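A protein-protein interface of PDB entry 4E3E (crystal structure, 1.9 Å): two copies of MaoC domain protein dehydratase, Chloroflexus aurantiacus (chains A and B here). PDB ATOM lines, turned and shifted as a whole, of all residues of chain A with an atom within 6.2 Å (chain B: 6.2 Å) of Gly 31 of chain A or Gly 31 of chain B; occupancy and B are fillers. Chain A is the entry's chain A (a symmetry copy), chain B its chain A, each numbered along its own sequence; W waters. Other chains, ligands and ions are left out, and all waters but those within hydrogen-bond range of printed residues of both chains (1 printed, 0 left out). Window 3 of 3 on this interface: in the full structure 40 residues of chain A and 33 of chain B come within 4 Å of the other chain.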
ATOM      1  N   THR A  29       9.440  26.924   8.748  1.00  0.00           N
ATOM      2  CA  THR A  29      10.274  26.723   7.552  1.00  0.00           C
ATOM      3  C   THR A  29      11.593  26.040   7.867  1.00  0.00           C
ATOM      4  O   THR A  29      11.946  25.835   9.042  1.00  0.00           O
ATOM      5  CB  THR A  29      10.626  28.059   6.885  1.00  0.00           C
ATOM      6  OG1 THR A  29      11.543  28.767   7.730  1.00  0.00           O
ATOM      7  CG2 THR A  29       9.387  28.914   6.692  1.00  0.00           C
ATOM      8  N   GLU A  30      12.353  25.766   6.808  1.00  0.00           N
ATOM      9  CA  GLU A  30      13.690  25.199   6.939  1.00  0.00           C
ATOM     10  C   GLU A  30      14.582  26.139   7.701  1.00  0.00           C
ATOM     11  O   GLU A  30      15.541  25.695   8.331  1.00  0.00           O
ATOM     12  CB  GLU A  30      14.301  24.863   5.568  1.00  0.00           C
ATOM     13  CG  GLU A  30      13.591  23.739   4.810  1.00  0.00           C
ATOM     14  CD  GLU A  30      13.927  22.328   5.322  1.00  0.00           C
ATOM     15  OE1 GLU A  30      14.302  22.156   6.519  1.00  0.00           O
ATOM     16  OE2 GLU A  30      13.807  21.370   4.516  1.00  0.00           O
ATOM     17  N   GLY A  31      14.278  27.436   7.675  1.00  0.00           N
ATOM     18  CA  GLY A  31      15.074  28.381   8.500  1.00  0.00           C
ATOM     19  C   GLY A  31      14.863  28.141   9.978  1.00  0.00           C
ATOM     20  O   GLY A  31      15.801  28.291  10.809  1.00  0.00           O
ATOM     21  N   ASP A  32      13.623  27.800  10.337  1.00  0.00           N
ATOM     22  CA  ASP A  32      13.314  27.464  11.741  1.00  0.00           C
ATOM     23  C   ASP A  32      14.028  26.184  12.156  1.00  0.00           C
ATOM     24  O   ASP A  32      14.586  26.095  13.252  1.00  0.00           O
ATOM     25  CB  ASP A  32      11.798  27.327  11.958  1.00  0.00           C
ATOM     26  CG  ASP A  32      11.071  28.611  11.665  1.00  0.00           C
ATOM     27  OD1 ASP A  32      11.439  29.667  12.258  1.00  0.00           O
ATOM     28  OD2 ASP A  32      10.139  28.571  10.838  1.00  0.00           O
ATOM     29  N   VAL A  33      14.011  25.200  11.268  1.00  0.00           N
ATOM     30  CA  VAL A  33      14.715  23.947  11.530  1.00  0.00           C
ATOM     31  C   VAL A  33      16.202  24.169  11.823  1.00  0.00           C
ATOM     32  O   VAL A  33      16.731  23.607  12.783  1.00  0.00           O
ATOM     33  CB  VAL A  33      14.560  22.982  10.359  1.00  0.00           C
ATOM     34  CG1 VAL A  33      15.477  21.767  10.541  1.00  0.00           C
ATOM     35  CG2 VAL A  33      13.098  22.565  10.233  1.00  0.00           C
ATOM     36  N   ALA A  34      16.878  24.982  10.999  1.00  0.00           N
ATOM     37  CA  ALA A  34      18.306  25.172  11.153  1.00  0.00           C
ATOM     38  C   ALA A  34      18.614  25.941  12.436  1.00  0.00           C
ATOM     39  O   ALA A  34      19.568  25.606  13.138  1.00  0.00           O
ATOM     40  CB  ALA A  34      18.899  25.887   9.938  1.00  0.00           C
ATOM     41  N   LEU A  35      17.799  26.957  12.748  1.00  0.00           N
ATOM     42  CA  LEU A  35      17.969  27.713  13.971  1.00  0.00           C
ATOM     43  C   LEU A  35      17.843  26.833  15.218  1.00  0.00           C
ATOM     44  O   LEU A  35      18.655  26.946  16.151  1.00  0.00           O
ATOM     45  CB  LEU A  35      16.956  28.867  14.035  1.00  0.00           C
ATOM     46  CG  LEU A  35      17.485  30.210  13.543  1.00  0.00           C
ATOM     47  CD1 LEU A  35      16.316  31.149  13.379  1.00  0.00           C
ATOM     48  CD2 LEU A  35      18.492  30.806  14.521  1.00  0.00           C
ATOM     49  N   TYR A  36      16.811  25.996  15.239  1.00  0.00           N
ATOM     50  CA  TYR A  36      16.569  25.050  16.339  1.00  0.00           C
ATOM     51  C   TYR A  36      17.780  24.107  16.507  1.00  0.00           C
ATOM     52  O   TYR A  36      18.277  23.901  17.621  1.00  0.00           O
ATOM     53  CB  TYR A  36      15.261  24.259  16.091  1.00  0.00           C
ATOM     54  CG  TYR A  36      14.845  23.427  17.291  1.00  0.00           C
ATOM     55  CD1 TYR A  36      14.148  24.011  18.355  1.00  0.00           C
ATOM     56  CD2 TYR A  36      15.196  22.069  17.389  1.00  0.00           C
ATOM     57  CE1 TYR A  36      13.781  23.260  19.470  1.00  0.00           C
ATOM     58  CE2 TYR A  36      14.843  21.309  18.506  1.00  0.00           C
ATOM     59  CZ  TYR A  36      14.143  21.915  19.549  1.00  0.00           C
ATOM     60  OH  TYR A  36      13.794  21.203  20.670  1.00  0.00           O
ATOM     61  N   LEU A 224      12.294  33.024  18.508  1.00  0.00           N
ATOM     62  CA  LEU A 224      11.932  32.098  17.424  1.00  0.00           C
ATOM     63  C   LEU A 224      10.510  31.583  17.674  1.00  0.00           C
ATOM     64  O   LEU A 224       9.724  31.390  16.733  1.00  0.00           O
ATOM     65  CB  LEU A 224      12.929  30.932  17.335  1.00  0.00           C
ATOM     66  CG  LEU A 224      12.660  29.877  16.249  1.00  0.00           C
ATOM     67  CD1 LEU A 224      12.850  30.472  14.856  1.00  0.00           C
ATOM     68  CD2 LEU A 224      13.547  28.653  16.427  1.00  0.00           C
ATOM     69  N   THR B  29      20.335  22.905   4.350  1.00  0.00           N
ATOM     70  CA  THR B  29      19.234  23.717   3.803  1.00  0.00           C
ATOM     71  C   THR B  29      19.580  25.193   3.726  1.00  0.00           C
ATOM     72  O   THR B  29      20.631  25.635   4.224  1.00  0.00           O
ATOM     73  CB  THR B  29      17.976  23.613   4.675  1.00  0.00           C
ATOM     74  OG1 THR B  29      18.217  24.294   5.913  1.00  0.00           O
ATOM     75  CG2 THR B  29      17.641  22.164   4.977  1.00  0.00           C
ATOM     76  N   GLU B  30      18.647  25.963   3.167  1.00  0.00           N
ATOM     77  CA  GLU B  30      18.778  27.414   3.099  1.00  0.00           C
ATOM     78  C   GLU B  30      18.844  27.996   4.483  1.00  0.00           C
ATOM     79  O   GLU B  30      19.420  29.067   4.668  1.00  0.00           O
ATOM     80  CB  GLU B  30      17.629  28.049   2.298  1.00  0.00           C
ATOM     81  CG  GLU B  30      17.617  27.697   0.808  1.00  0.00           C
ATOM     82  CD  GLU B  30      18.650  28.473  -0.027  1.00  0.00           C
ATOM     83  OE1 GLU B  30      19.700  28.925   0.515  1.00  0.00           O
ATOM     84  OE2 GLU B  30      18.411  28.628  -1.253  1.00  0.00           O
ATOM     85  N   GLY B  31      18.280  27.303   5.472  1.00  0.00           N
ATOM     86  CA  GLY B  31      18.417  27.796   6.867  1.00  0.00           C
ATOM     87  C   GLY B  31      19.850  27.722   7.344  1.00  0.00           C
ATOM     88  O   GLY B  31      20.331  28.596   8.117  1.00  0.00           O
ATOM     89  N   ASP B  32      20.546  26.664   6.923  1.00  0.00           N
ATOM     90  CA  ASP B  32      21.977  26.525   7.259  1.00  0.00           C
ATOM     91  C   ASP B  32      22.796  27.615   6.580  1.00  0.00           C
ATOM     92  O   ASP B  32      23.687  28.212   7.188  1.00  0.00           O
ATOM     93  CB  ASP B  32      22.506  25.135   6.868  1.00  0.00           C
ATOM     94  CG  ASP B  32      21.794  24.034   7.607  1.00  0.00           C
ATOM     95  OD1 ASP B  32      21.756  24.077   8.872  1.00  0.00           O
ATOM     96  OD2 ASP B  32      21.264  23.132   6.929  1.00  0.00           O
ATOM     97  N   VAL B  33      22.480  27.873   5.319  1.00  0.00           N
ATOM     98  CA  VAL B  33      23.155  28.940   4.584  1.00  0.00           C
ATOM     99  C   VAL B  33      23.035  30.293   5.290  1.00  0.00           C
ATOM    100  O   VAL B  33      24.032  31.005   5.431  1.00  0.00           O
ATOM    101  CB  VAL B  33      22.609  29.051   3.164  1.00  0.00           C
ATOM    102  CG1 VAL B  33      23.158  30.305   2.476  1.00  0.00           C
ATOM    103  CG2 VAL B  33      22.958  27.787   2.384  1.00  0.00           C
ATOM    104  N   ALA B  34      21.822  30.653   5.731  1.00  0.00           N
ATOM    105  CA  ALA B  34      21.606  31.956   6.327  1.00  0.00           C
ATOM    106  C   ALA B  34      22.312  32.056   7.679  1.00  0.00           C
ATOM    107  O   ALA B  34      22.901  33.091   7.988  1.00  0.00           O
ATOM    108  CB  ALA B  34      20.113  32.255   6.473  1.00  0.00           C
ATOM    109  N   LEU B  35      22.264  30.977   8.471  1.00  0.00           N
ATOM    110  CA  LEU B  35      22.948  30.949   9.747  1.00  0.00           C
ATOM    111  C   LEU B  35      24.458  31.146   9.599  1.00  0.00           C
ATOM    112  O   LEU B  35      25.070  31.916  10.359  1.00  0.00           O
ATOM    113  CB  LEU B  35      22.658  29.629  10.482  1.00  0.00           C
ATOM    114  CG  LEU B  35      21.517  29.697  11.490  1.00  0.00           C
ATOM    115  CD1 LEU B  35      21.156  28.289  11.894  1.00  0.00           C
ATOM    116  CD2 LEU B  35      21.908  30.503  12.724  1.00  0.00           C
ATOM    117  N   TYR B  36      25.051  30.426   8.651  1.00  0.00           N
ATOM    118  CA  TYR B  36      26.487  30.530   8.346  1.00  0.00           C
ATOM    119  C   TYR B  36      26.845  31.979   7.951  1.00  0.00           C
ATOM    120  O   TYR B  36      27.817  32.555   8.456  1.00  0.00           O
ATOM    121  CB  TYR B  36      26.874  29.524   7.234  1.00  0.00           C
ATOM    122  CG  TYR B  36      28.376  29.431   7.028  1.00  0.00           C
ATOM    123  CD1 TYR B  36      29.159  28.626   7.862  1.00  0.00           C
ATOM    124  CD2 TYR B  36      29.021  30.189   6.037  1.00  0.00           C
ATOM    125  CE1 TYR B  36      30.540  28.550   7.696  1.00  0.00           C
ATOM    126  CE2 TYR B  36      30.406  30.130   5.866  1.00  0.00           C
ATOM    127  CZ  TYR B  36      31.161  29.314   6.708  1.00  0.00           C
ATOM    128  OH  TYR B  36      32.527  29.243   6.580  1.00  0.00           O
ATOM    129  N   LEU B 224      25.487  24.069  14.966  1.00  0.00           N
ATOM    130  CA  LEU B 224      25.037  23.975  13.568  1.00  0.00           C
ATOM    131  C   LEU B 224      25.752  22.793  12.903  1.00  0.00           C
ATOM    132  O   LEU B 224      25.166  22.073  12.079  1.00  0.00           O
ATOM    133  CB  LEU B 224      25.313  25.281  12.808  1.00  0.00           C
ATOM    134  CG  LEU B 224      24.904  25.314  11.325  1.00  0.00           C
ATOM    135  CD1 LEU B 224      23.386  25.260  11.181  1.00  0.00           C
ATOM    136  CD2 LEU B 224      25.459  26.544  10.620  1.00  0.00           C
HETATM  137  O   HOH W   1      16.740  23.367   7.787  1.00  0.00           O
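The side-chain hydroxyl of Thr 29 of chain A sits close to the backbone NH of Gly 31 of chain A, at 3.0 Å. The backbone NH (N) of Thr 29 of chain B sits at hydrogen-bond distance from the side-chain carboxylate (OD2) of Asp 32 of chain B (2.8 Å). The side-chain hydroxyl (OG1) of Thr 29 of chain B sits close to the backbone NH (N) of Gly 31 of chain B (3.0 Å).
Glu 30 of chain A touches Thr 29 of chain B. Gly 31 of chain B touches Glu 30 of chain A. CA of Gly 31 of chain A touches CA of Gly 31 of chain B, at 3.8 Å. CB of Ala 34 of chain A touches C of Gly 31 of chain B, 3.3 Å away. Ala 34 of chain A touches Asp 32 of chain B (CB to N, 3.5 Å). Ala 34 of chain A touches Leu 35 of chain B. Leu 35 of chain A touches Leu 35 of chain B (N to CD1, 3.7 Å).
Printed residues of chain B within 4 Å of Glu 30 of chain A: Thr 29 and Gly 31. Of chain B, only Gly 31 comes within 4 Å of Gly 31 of chain A. Of the printed residues of chain B, Leu 35 of chain A touches Leu 35. Gly 31 of chain B touches just these residues of chain A: Glu 30, Gly 31 and Ala 34. Of the printed residues of chain A, Asp 32 of chain B touches Ala 34 (3.5 Å). Of the printed residues of chain A, Leu 35 of chain B touches Ala 34 and Leu 35. The nearest residue of chain A that does not touch Gly 31 of chain B is Leu 35 of chain A (5.5 Å). The nearest printed residue of chain B that does not touch Glu 30 of chain A is Glu 30 of chain B (5.1 Å).
Of the 9 printed residues of chain A, 4 touch a printed residue of chain B. Hydrophobic or aromatic side chains of chain A within 4 Å of the printed part of chain B: Ala 34 and Leu 35. Of the 9 printed residues of chain B, 4 touch a printed residue of chain A. Hydrophobic or aromatic side chains of chain B within 4 Å of the printed part of chain A: Leu 35. Among the printed residues, no Asp or Glu carboxylate lies within 4 Å of a Lys or Arg side-chain nitrogen of the other chain.
Glu 30 of chain A touches Thr 29 of chain B, but with the chains exchanged Thr 29 of chain A does not touch Glu 30 of chain B (8.0 Å). Glu 30 of chain A touches Gly 31 of chain B, but with the chains exchanged Gly 31 of chain A does not touch Glu 30 of chain B (5.5 Å). Gly 31 of chain A touches its own counterpart, Gly 31 of chain B. Ala 34 of chain A touches Asp 32 of chain B, but with the chains exchanged Asp 32 of chain A does not touch Ala 34 of chain B (8.8 Å). 9 positions are printed for both chains. Of the 7 pairs that touch across the chains among the printed residues, 2 have their exchanged pair printed and touching as well.
Water W1 bridges the side-chain hydroxyl of Thr 29 of chain B and the backbone carbonyl oxygen of Glu 30 of chain A.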
